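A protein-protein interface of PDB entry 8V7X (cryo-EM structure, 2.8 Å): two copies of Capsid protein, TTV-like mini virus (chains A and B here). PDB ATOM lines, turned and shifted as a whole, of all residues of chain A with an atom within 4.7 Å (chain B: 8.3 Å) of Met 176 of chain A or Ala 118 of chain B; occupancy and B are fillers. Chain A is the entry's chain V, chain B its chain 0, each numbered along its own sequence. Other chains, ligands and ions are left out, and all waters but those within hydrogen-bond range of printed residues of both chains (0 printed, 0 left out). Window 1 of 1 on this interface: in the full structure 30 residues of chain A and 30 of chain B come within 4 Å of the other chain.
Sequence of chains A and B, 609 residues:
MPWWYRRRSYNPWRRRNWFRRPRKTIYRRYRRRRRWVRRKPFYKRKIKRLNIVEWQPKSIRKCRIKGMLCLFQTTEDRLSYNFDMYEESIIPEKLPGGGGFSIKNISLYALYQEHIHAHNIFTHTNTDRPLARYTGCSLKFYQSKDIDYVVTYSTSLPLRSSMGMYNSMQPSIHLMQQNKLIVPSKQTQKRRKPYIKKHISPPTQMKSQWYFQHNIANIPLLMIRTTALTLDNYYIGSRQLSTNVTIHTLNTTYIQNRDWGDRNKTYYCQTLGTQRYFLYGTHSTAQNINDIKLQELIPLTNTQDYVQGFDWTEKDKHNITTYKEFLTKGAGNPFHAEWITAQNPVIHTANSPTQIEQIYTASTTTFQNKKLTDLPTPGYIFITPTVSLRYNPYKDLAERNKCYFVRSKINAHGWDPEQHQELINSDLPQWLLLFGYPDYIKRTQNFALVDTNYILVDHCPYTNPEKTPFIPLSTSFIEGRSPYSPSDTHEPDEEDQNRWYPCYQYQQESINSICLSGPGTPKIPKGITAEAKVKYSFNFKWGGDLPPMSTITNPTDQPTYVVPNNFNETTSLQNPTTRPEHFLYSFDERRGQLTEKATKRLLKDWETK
The backbone NH of Asn 120 of chain B lies close to the side-chain sulfur of Met 176 of chain A (3.5 Å).
O of Ala 118 of chain B sits close to SD of Met 176 of chain A, at 3.8 Å.
The side-chain sulfur (SD) of Met 176 of chain A sits close to the backbone carbonyl oxygen (O) of His 119 of chain B (3.5 Å).
The backbone carbonyl oxygen (O) of Lys 66 of chain B lies within hydrogen-bond range of the backbone NH (N) of Ile 121 of chain B (2.9 Å).
The backbone NH (N) of Met 68 of chain B is in hydrogen-bond range of the backbone carbonyl oxygen (O) of His 119 of chain B.
The backbone carbonyl oxygen (O) of Leu 111 of chain B sits at hydrogen-bond distance from the side-chain amide nitrogen (ND2) of Asn 120 of chain B (2.9 Å).
The side-chain carboxylate of Glu 114 of chain B sits at hydrogen-bond distance from a ring nitrogen (ND1) of His 119 of chain B (2.8 Å).
A ring nitrogen (ND1) of His 115 of chain B lies within hydrogen-bond range of the side-chain amide oxygen of Asn 120 of chain B, at 3.0 Å.
ND2 of Asn 120 of chain B is in hydrogen-bond range of OH of Tyr 536 of chain B, at 3.0 Å.
Ala 118 of chain B touches Ile 173 of chain A.
Met 68 of chain B touches Leu 175 of chain A.
Ile 121 of chain B touches Met 176 of chain A.
His 117 of chain B touches Trp 431 of chain A (O to CZ2, 3.2 Å).
Leu 432 of chain A touches Ala 118 of chain B.
His 174 of chain A touches none of the printed residues of chain B.
Of the printed residues of chain B, Leu 175 of chain A touches Met 68 (3.6 Å).
Printed residues of chain B within 4 Å of Met 176 of chain A: Ala 118, His 119, Asn 120 and Ile 121.
Of the printed residues of chain B, Trp 431 of chain A touches His 117 (3.2 Å).
Printed residues of chain A within 4 Å of Met 68 of chain B: Leu 175.
Ala 118 of chain B touches just these residues of chain A: Ile 173, Met 176 and Leu 432.
Of the printed residues of chain A, Ile 121 of chain B touches Met 176.
The nearest residue of chain B that does not touch Met 176 of chain A is Lys 66 of chain B (4.5 Å).
The nearest residue of chain A that does not touch Ala 118 of chain B is Trp 431 of chain A (4.1 Å).
Printed residues of chain A that touch a printed residue of chain B: Ile 173, Leu 175, Met 176, Trp 431 and Leu 432.
Hydrophobic or aromatic side chains of chain A within 4 Å of the printed part of chain B: Ile 173, Leu 175, Met 176, Trp 431 and Leu 432.
Along chain A the printed residues that touch a printed residue of chain B span positions 173 to 432.
Among the printed residues, 8 pairs touch across the chains.
No position is printed for both chains.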
ATOM      1  N   SER A 172      27.823  21.014 -18.557  1.00  0.00           N
ATOM      2  CA  SER A 172      26.604  21.660 -19.042  1.00  0.00           C
ATOM      3  C   SER A 172      25.534  21.760 -17.952  1.00  0.00           C
ATOM      4  O   SER A 172      24.912  22.803 -17.784  1.00  0.00           O
ATOM      5  CB  SER A 172      26.091  20.863 -20.240  1.00  0.00           C
ATOM      6  OG  SER A 172      24.904  21.415 -20.738  1.00  0.00           O
ATOM      7  N   ILE A 173      25.359  20.706 -17.153  1.00  0.00           N
ATOM      8  CA  ILE A 173      24.379  20.679 -16.069  1.00  0.00           C
ATOM      9  C   ILE A 173      24.794  21.598 -14.926  1.00  0.00           C
ATOM     10  O   ILE A 173      23.985  22.389 -14.458  1.00  0.00           O
ATOM     11  CB  ILE A 173      24.139  19.242 -15.583  1.00  0.00           C
ATOM     12  CG1 ILE A 173      23.800  18.278 -16.734  1.00  0.00           C
ATOM     13  CG2 ILE A 173      23.024  19.215 -14.531  1.00  0.00           C
ATOM     14  CD1 ILE A 173      22.709  18.723 -17.705  1.00  0.00           C
ATOM     15  N   HIS A 174      26.059  21.560 -14.516  1.00  0.00           N
ATOM     16  CA  HIS A 174      26.594  22.454 -13.500  1.00  0.00           C
ATOM     17  C   HIS A 174      26.483  23.915 -13.955  1.00  0.00           C
ATOM     18  O   HIS A 174      26.012  24.763 -13.209  1.00  0.00           O
ATOM     19  CB  HIS A 174      28.037  22.036 -13.203  1.00  0.00           C
ATOM     20  CG  HIS A 174      28.641  22.566 -11.923  1.00  0.00           C
ATOM     21  ND1 HIS A 174      29.797  22.100 -11.350  1.00  0.00           N
ATOM     22  CD2 HIS A 174      28.230  23.627 -11.163  1.00  0.00           C
ATOM     23  CE1 HIS A 174      30.089  22.873 -10.299  1.00  0.00           C
ATOM     24  NE2 HIS A 174      29.162  23.819 -10.148  1.00  0.00           N
ATOM     25  N   LEU A 175      26.812  24.223 -15.208  1.00  0.00           N
ATOM     26  CA  LEU A 175      26.641  25.560 -15.769  1.00  0.00           C
ATOM     27  C   LEU A 175      25.177  26.043 -15.797  1.00  0.00           C
ATOM     28  O   LEU A 175      24.940  27.245 -15.787  1.00  0.00           O
ATOM     29  CB  LEU A 175      27.309  25.569 -17.150  1.00  0.00           C
ATOM     30  CG  LEU A 175      27.262  26.933 -17.853  1.00  0.00           C
ATOM     31  CD1 LEU A 175      28.603  27.247 -18.487  1.00  0.00           C
ATOM     32  CD2 LEU A 175      26.215  26.947 -18.967  1.00  0.00           C
ATOM     33  N   MET A 176      24.175  25.167 -15.796  1.00  0.00           N
ATOM     34  CA  MET A 176      22.774  25.586 -15.676  1.00  0.00           C
ATOM     35  C   MET A 176      22.324  25.880 -14.244  1.00  0.00           C
ATOM     36  O   MET A 176      21.319  26.563 -14.058  1.00  0.00           O
ATOM     37  CB  MET A 176      21.852  24.533 -16.287  1.00  0.00           C
ATOM     38  CG  MET A 176      21.938  24.555 -17.809  1.00  0.00           C
ATOM     39  SD  MET A 176      20.754  23.472 -18.626  1.00  0.00           S
ATOM     40  CE  MET A 176      21.342  21.849 -18.113  1.00  0.00           C
ATOM     41  N   GLN A 177      23.011  25.378 -13.218  1.00  0.00           N
ATOM     42  CA  GLN A 177      22.565  25.522 -11.829  1.00  0.00           C
ATOM     43  C   GLN A 177      22.535  26.973 -11.346  1.00  0.00           C
ATOM     44  O   GLN A 177      23.289  27.828 -11.804  1.00  0.00           O
ATOM     45  CB  GLN A 177      23.415  24.647 -10.900  1.00  0.00           C
ATOM     46  CG  GLN A 177      23.023  23.177 -11.080  1.00  0.00           C
ATOM     47  CD  GLN A 177      23.846  22.223 -10.232  1.00  0.00           C
ATOM     48  OE1 GLN A 177      25.012  22.429  -9.941  1.00  0.00           O
ATOM     49  NE2 GLN A 177      23.258  21.130  -9.800  1.00  0.00           N
ATOM     50  N   GLN A 178      21.658  27.258 -10.382  1.00  0.00           N
ATOM     51  CA  GLN A 178      21.616  28.547  -9.694  1.00  0.00           C
ATOM     52  C   GLN A 178      22.777  28.690  -8.709  1.00  0.00           C
ATOM     53  O   GLN A 178      23.267  27.706  -8.155  1.00  0.00           O
ATOM     54  CB  GLN A 178      20.285  28.732  -8.951  1.00  0.00           C
ATOM     55  CG  GLN A 178      19.093  28.885  -9.911  1.00  0.00           C
ATOM     56  CD  GLN A 178      17.856  29.497  -9.250  1.00  0.00           C
ATOM     57  OE1 GLN A 178      17.817  29.802  -8.063  1.00  0.00           O
ATOM     58  NE2 GLN A 178      16.794  29.712 -10.001  1.00  0.00           N
ATOM     59  N   TRP A 431      25.721  10.293 -21.765  1.00  0.00           N
ATOM     60  CA  TRP A 431      26.776  11.246 -21.429  1.00  0.00           C
ATOM     61  C   TRP A 431      26.547  11.943 -20.083  1.00  0.00           C
ATOM     62  O   TRP A 431      27.509  12.335 -19.439  1.00  0.00           O
ATOM     63  CB  TRP A 431      26.920  12.254 -22.571  1.00  0.00           C
ATOM     64  CG  TRP A 431      25.702  13.064 -22.905  1.00  0.00           C
ATOM     65  CD1 TRP A 431      24.866  12.811 -23.932  1.00  0.00           C
ATOM     66  CD2 TRP A 431      25.155  14.246 -22.238  1.00  0.00           C
ATOM     67  NE1 TRP A 431      23.845  13.734 -23.940  1.00  0.00           N
ATOM     68  CE2 TRP A 431      23.962  14.630 -22.911  1.00  0.00           C
ATOM     69  CE3 TRP A 431      25.542  15.036 -21.137  1.00  0.00           C
ATOM     70  CZ2 TRP A 431      23.181  15.717 -22.504  1.00  0.00           C
ATOM     71  CZ3 TRP A 431      24.764  16.130 -20.715  1.00  0.00           C
ATOM     72  CH2 TRP A 431      23.586  16.471 -21.394  1.00  0.00           C
ATOM     73  N   LEU A 432      25.300  12.081 -19.632  1.00  0.00           N
ATOM     74  CA  LEU A 432      24.957  12.561 -18.299  1.00  0.00           C
ATOM     75  C   LEU A 432      24.867  11.415 -17.289  1.00  0.00           C
ATOM     76  O   LEU A 432      25.301  11.559 -16.155  1.00  0.00           O
ATOM     77  CB  LEU A 432      23.640  13.336 -18.391  1.00  0.00           C
ATOM     78  CG  LEU A 432      23.143  13.885 -17.051  1.00  0.00           C
ATOM     79  CD1 LEU A 432      24.187  14.733 -16.339  1.00  0.00           C
ATOM     80  CD2 LEU A 432      21.916  14.748 -17.301  1.00  0.00           C
ATOM     81  N   LYS B  66      15.542  28.514 -18.932  1.00  0.00           N
ATOM     82  CA  LYS B  66      16.901  28.995 -19.216  1.00  0.00           C
ATOM     83  C   LYS B  66      17.743  27.889 -19.819  1.00  0.00           C
ATOM     84  O   LYS B  66      17.752  26.787 -19.289  1.00  0.00           O
ATOM     85  CB  LYS B  66      17.584  29.469 -17.932  1.00  0.00           C
ATOM     86  CG  LYS B  66      17.062  30.792 -17.384  1.00  0.00           C
ATOM     87  CD  LYS B  66      17.806  31.107 -16.083  1.00  0.00           C
ATOM     88  CE  LYS B  66      17.445  32.499 -15.572  1.00  0.00           C
ATOM     89  NZ  LYS B  66      18.127  32.788 -14.285  1.00  0.00           N
ATOM     90  N   GLY B  67      18.498  28.166 -20.869  1.00  0.00           N
ATOM     91  CA  GLY B  67      19.343  27.154 -21.496  1.00  0.00           C
ATOM     92  C   GLY B  67      20.238  27.695 -22.593  1.00  0.00           C
ATOM     93  O   GLY B  67      20.328  28.896 -22.804  1.00  0.00           O
ATOM     94  N   MET B  68      20.909  26.792 -23.292  1.00  0.00           N
ATOM     95  CA  MET B  68      21.888  27.094 -24.331  1.00  0.00           C
ATOM     96  C   MET B  68      21.472  26.424 -25.644  1.00  0.00           C
ATOM     97  O   MET B  68      21.140  25.245 -25.642  1.00  0.00           O
ATOM     98  CB  MET B  68      23.251  26.584 -23.840  1.00  0.00           C
ATOM     99  CG  MET B  68      24.453  27.282 -24.470  1.00  0.00           C
ATOM    100  SD  MET B  68      24.840  28.921 -23.800  1.00  0.00           S
ATOM    101  CE  MET B  68      25.278  28.518 -22.095  1.00  0.00           C
ATOM    102  N   TYR B  86      19.398  17.547 -34.848  1.00  0.00           N
ATOM    103  CA  TYR B  86      18.745  16.245 -34.877  1.00  0.00           C
ATOM    104  C   TYR B  86      18.590  15.821 -36.345  1.00  0.00           C
ATOM    105  O   TYR B  86      17.852  16.420 -37.124  1.00  0.00           O
ATOM    106  CB  TYR B  86      17.436  16.355 -34.090  1.00  0.00           C
ATOM    107  CG  TYR B  86      17.632  16.945 -32.699  1.00  0.00           C
ATOM    108  CD1 TYR B  86      18.477  16.298 -31.779  1.00  0.00           C
ATOM    109  CD2 TYR B  86      17.041  18.174 -32.350  1.00  0.00           C
ATOM    110  CE1 TYR B  86      18.742  16.877 -30.527  1.00  0.00           C
ATOM    111  CE2 TYR B  86      17.293  18.751 -31.091  1.00  0.00           C
ATOM    112  CZ  TYR B  86      18.150  18.105 -30.176  1.00  0.00           C
ATOM    113  OH  TYR B  86      18.405  18.648 -28.960  1.00  0.00           O
ATOM    114  N   LEU B 111      11.059  23.487 -26.231  1.00  0.00           N
ATOM    115  CA  LEU B 111      11.719  23.736 -24.951  1.00  0.00           C
ATOM    116  C   LEU B 111      11.614  22.543 -23.997  1.00  0.00           C
ATOM    117  O   LEU B 111      12.602  22.199 -23.357  1.00  0.00           O
ATOM    118  CB  LEU B 111      11.144  24.995 -24.293  1.00  0.00           C
ATOM    119  CG  LEU B 111      11.479  26.301 -25.019  1.00  0.00           C
ATOM    120  CD1 LEU B 111      10.780  27.471 -24.336  1.00  0.00           C
ATOM    121  CD2 LEU B 111      12.979  26.582 -25.029  1.00  0.00           C
ATOM    122  N   TYR B 112      10.466  21.873 -23.927  1.00  0.00           N
ATOM    123  CA  TYR B 112      10.329  20.617 -23.199  1.00  0.00           C
ATOM    124  C   TYR B 112      11.205  19.505 -23.787  1.00  0.00           C
ATOM    125  O   TYR B 112      11.860  18.786 -23.045  1.00  0.00           O
ATOM    126  CB  TYR B 112       8.849  20.227 -23.158  1.00  0.00           C
ATOM    127  CG  TYR B 112       8.608  18.806 -22.709  1.00  0.00           C
ATOM    128  CD1 TYR B 112       8.591  18.494 -21.339  1.00  0.00           C
ATOM    129  CD2 TYR B 112       8.475  17.788 -23.668  1.00  0.00           C
ATOM    130  CE1 TYR B 112       8.453  17.157 -20.929  1.00  0.00           C
ATOM    131  CE2 TYR B 112       8.352  16.451 -23.259  1.00  0.00           C
ATOM    132  CZ  TYR B 112       8.341  16.136 -21.888  1.00  0.00           C
ATOM    133  OH  TYR B 112       8.223  14.844 -21.491  1.00  0.00           O
ATOM    134  N   GLN B 113      11.296  19.367 -25.108  1.00  0.00           N
ATOM    135  CA  GLN B 113      12.199  18.397 -25.727  1.00  0.00           C
ATOM    136  C   GLN B 113      13.670  18.692 -25.419  1.00  0.00           C
ATOM    137  O   GLN B 113      14.428  17.773 -25.129  1.00  0.00           O
ATOM    138  CB  GLN B 113      11.959  18.358 -27.235  1.00  0.00           C
ATOM    139  CG  GLN B 113      10.632  17.679 -27.587  1.00  0.00           C
ATOM    140  CD  GLN B 113      10.453  17.550 -29.095  1.00  0.00           C
ATOM    141  OE1 GLN B 113      10.590  18.495 -29.857  1.00  0.00           O
ATOM    142  NE2 GLN B 113      10.160  16.370 -29.595  1.00  0.00           N
ATOM    143  N   GLU B 114      14.092  19.953 -25.404  1.00  0.00           N
ATOM    144  CA  GLU B 114      15.438  20.328 -24.967  1.00  0.00           C
ATOM    145  C   GLU B 114      15.676  20.024 -23.482  1.00  0.00           C
ATOM    146  O   GLU B 114      16.792  19.670 -23.115  1.00  0.00           O
ATOM    147  CB  GLU B 114      15.686  21.813 -25.266  1.00  0.00           C
ATOM    148  CG  GLU B 114      15.841  22.142 -26.754  1.00  0.00           C
ATOM    149  CD  GLU B 114      16.987  21.372 -27.421  1.00  0.00           C
ATOM    150  OE1 GLU B 114      18.165  21.669 -27.133  1.00  0.00           O
ATOM    151  OE2 GLU B 114      16.713  20.475 -28.246  1.00  0.00           O
ATOM    152  N   HIS B 115      14.628  19.981 -22.655  1.00  0.00           N
ATOM    153  CA  HIS B 115      14.751  19.585 -21.224  1.00  0.00           C
ATOM    154  C   HIS B 115      14.990  18.075 -21.122  1.00  0.00           C
ATOM    155  O   HIS B 115      15.592  17.662 -20.117  1.00  0.00           O
ATOM    156  CB  HIS B 115      13.500  19.988 -20.445  1.00  0.00           C
ATOM    157  CG  HIS B 115      13.698  20.016 -18.970  1.00  0.00           C
ATOM    158  ND1 HIS B 115      14.269  21.078 -18.308  1.00  0.00           N
ATOM    159  CD2 HIS B 115      13.404  19.109 -18.036  1.00  0.00           C
ATOM    160  CE1 HIS B 115      14.308  20.812 -17.012  1.00  0.00           C
ATOM    161  NE2 HIS B 115      13.789  19.619 -16.825  1.00  0.00           N
ATOM    162  N   ILE B 116      14.455  17.281 -22.052  1.00  0.00           N
ATOM    163  CA  ILE B 116      14.730  15.835 -22.103  1.00  0.00           C
ATOM    164  C   ILE B 116      16.184  15.551 -22.506  1.00  0.00           C
ATOM    165  O   ILE B 116      16.789  14.602 -22.015  1.00  0.00           O
ATOM    166  CB  ILE B 116      13.720  15.110 -23.025  1.00  0.00           C
ATOM    167  CG1 ILE B 116      12.256  15.299 -22.586  1.00  0.00           C
ATOM    168  CG2 ILE B 116      14.022  13.611 -23.135  1.00  0.00           C
ATOM    169  CD1 ILE B 116      11.952  14.922 -21.134  1.00  0.00           C
ATOM    170  N   HIS B 117      16.791  16.402 -23.331  1.00  0.00           N
ATOM    171  CA  HIS B 117      18.231  16.373 -23.621  1.00  0.00           C
ATOM    172  C   HIS B 117      19.099  17.010 -22.525  1.00  0.00           C
ATOM    173  O   HIS B 117      20.316  17.066 -22.664  1.00  0.00           O
ATOM    174  CB  HIS B 117      18.481  17.014 -24.990  1.00  0.00           C
ATOM    175  CG  HIS B 117      18.046  16.154 -26.144  1.00  0.00           C
ATOM    176  ND1 HIS B 117      18.743  15.045 -26.624  1.00  0.00           N
ATOM    177  CD2 HIS B 117      16.930  16.329 -26.902  1.00  0.00           C
ATOM    178  CE1 HIS B 117      18.037  14.584 -27.666  1.00  0.00           C
ATOM    179  NE2 HIS B 117      16.940  15.332 -27.850  1.00  0.00           N
ATOM    180  N   ALA B 118      18.507  17.482 -21.427  1.00  0.00           N
ATOM    181  CA  ALA B 118      19.165  18.227 -20.357  1.00  0.00           C
ATOM    182  C   ALA B 118      19.841  19.532 -20.822  1.00  0.00           C
ATOM    183  O   ALA B 118      20.777  20.011 -20.188  1.00  0.00           O
ATOM    184  CB  ALA B 118      20.070  17.292 -19.545  1.00  0.00           C
ATOM    185  N   HIS B 119      19.390  20.128 -21.925  1.00  0.00           N
ATOM    186  CA  HIS B 119      19.953  21.365 -22.465  1.00  0.00           C
ATOM    187  C   HIS B 119      19.405  22.634 -21.803  1.00  0.00           C
ATOM    188  O   HIS B 119      19.946  23.718 -22.014  1.00  0.00           O
ATOM    189  CB  HIS B 119      19.728  21.404 -23.978  1.00  0.00           C
ATOM    190  CG  HIS B 119      20.437  20.341 -24.781  1.00  0.00           C
ATOM    191  ND1 HIS B 119      20.176  20.060 -26.095  1.00  0.00           N
ATOM    192  CD2 HIS B 119      21.517  19.582 -24.422  1.00  0.00           C
ATOM    193  CE1 HIS B 119      21.056  19.145 -26.522  1.00  0.00           C
ATOM    194  NE2 HIS B 119      21.909  18.825 -25.533  1.00  0.00           N
ATOM    195  N   ASN B 120      18.352  22.534 -20.994  1.00  0.00           N
ATOM    196  CA  ASN B 120      17.789  23.658 -20.255  1.00  0.00           C
ATOM    197  C   ASN B 120      17.286  23.252 -18.869  1.00  0.00           C
ATOM    198  O   ASN B 120      17.147  22.073 -18.558  1.00  0.00           O
ATOM    199  CB  ASN B 120      16.726  24.385 -21.101  1.00  0.00           C
ATOM    200  CG  ASN B 120      15.513  23.571 -21.477  1.00  0.00           C
ATOM    201  OD1 ASN B 120      15.039  22.748 -20.732  1.00  0.00           O
ATOM    202  ND2 ASN B 120      14.954  23.793 -22.631  1.00  0.00           N
ATOM    203  N   ILE B 121      17.034  24.259 -18.042  1.00  0.00           N
ATOM    204  CA  ILE B 121      16.331  24.147 -16.768  1.00  0.00           C
ATOM    205  C   ILE B 121      14.996  24.882 -16.862  1.00  0.00           C
ATOM    206  O   ILE B 121      14.888  25.919 -17.512  1.00  0.00           O
ATOM    207  CB  ILE B 121      17.179  24.680 -15.593  1.00  0.00           C
ATOM    208  CG1 ILE B 121      17.506  26.184 -15.688  1.00  0.00           C
ATOM    209  CG2 ILE B 121      18.458  23.849 -15.433  1.00  0.00           C
ATOM    210  CD1 ILE B 121      17.926  26.802 -14.359  1.00  0.00           C
ATOM    211  N   PHE B 122      13.984  24.390 -16.157  1.00  0.00           N
ATOM    212  CA  PHE B 122      12.765  25.141 -15.868  1.00  0.00           C
ATOM    213  C   PHE B 122      12.875  25.636 -14.429  1.00  0.00           C
ATOM    214  O   PHE B 122      12.990  24.840 -13.502  1.00  0.00           O
ATOM    215  CB  PHE B 122      11.530  24.247 -16.040  1.00  0.00           C
ATOM    216  CG  PHE B 122      11.033  24.015 -17.456  1.00  0.00           C
ATOM    217  CD1 PHE B 122      11.867  23.479 -18.455  1.00  0.00           C
ATOM    218  CD2 PHE B 122       9.685  24.273 -17.757  1.00  0.00           C
ATOM    219  CE1 PHE B 122      11.361  23.225 -19.739  1.00  0.00           C
ATOM    220  CE2 PHE B 122       9.177  24.006 -19.037  1.00  0.00           C
ATOM    221  CZ  PHE B 122      10.015  23.481 -20.031  1.00  0.00           C
ATOM    222  N   THR B 123      12.839  26.949 -14.220  1.00  0.00           N
ATOM    223  CA  THR B 123      12.995  27.542 -12.878  1.00  0.00           C
ATOM    224  C   THR B 123      11.866  27.156 -11.914  1.00  0.00           C
ATOM    225  O   THR B 123      12.086  27.064 -10.711  1.00  0.00           O
ATOM    226  CB  THR B 123      13.125  29.064 -12.999  1.00  0.00           C
ATOM    227  OG1 THR B 123      14.345  29.376 -13.626  1.00  0.00           O
ATOM    228  CG2 THR B 123      13.119  29.835 -11.686  1.00  0.00           C
ATOM    229  N   LYS B 535      22.558  31.853 -25.448  1.00  0.00           N
ATOM    230  CA  LYS B 535      21.870  31.521 -24.201  1.00  0.00           C
ATOM    231  C   LYS B 535      20.512  32.194 -24.204  1.00  0.00           C
ATOM    232  O   LYS B 535      20.422  33.400 -24.398  1.00  0.00           O
ATOM    233  CB  LYS B 535      22.709  31.912 -22.978  1.00  0.00           C
ATOM    234  CG  LYS B 535      22.099  31.329 -21.700  1.00  0.00           C
ATOM    235  CD  LYS B 535      22.876  31.660 -20.430  1.00  0.00           C
ATOM    236  CE  LYS B 535      22.178  30.941 -19.268  1.00  0.00           C
ATOM    237  NZ  LYS B 535      22.948  31.062 -18.003  1.00  0.00           N
ATOM    238  N   TYR B 536      19.459  31.426 -23.989  1.00  0.00           N
ATOM    239  CA  TYR B 536      18.090  31.917 -23.987  1.00  0.00           C
ATOM    240  C   TYR B 536      17.498  31.904 -22.587  1.00  0.00           C
ATOM    241  O   TYR B 536      17.894  31.124 -21.727  1.00  0.00           O
ATOM    242  CB  TYR B 536      17.233  31.125 -24.973  1.00  0.00           C
ATOM    243  CG  TYR B 536      17.133  29.639 -24.724  1.00  0.00           C
ATOM    244  CD1 TYR B 536      16.309  29.134 -23.701  1.00  0.00           C
ATOM    245  CD2 TYR B 536      17.826  28.755 -25.562  1.00  0.00           C
ATOM    246  CE1 TYR B 536      16.168  27.749 -23.526  1.00  0.00           C
ATOM    247  CE2 TYR B 536      17.681  27.372 -25.391  1.00  0.00           C
ATOM    248  CZ  TYR B 536      16.842  26.869 -24.387  1.00  0.00           C
ATOM    249  OH  TYR B 536      16.689  25.530 -24.280  1.00  0.00           O
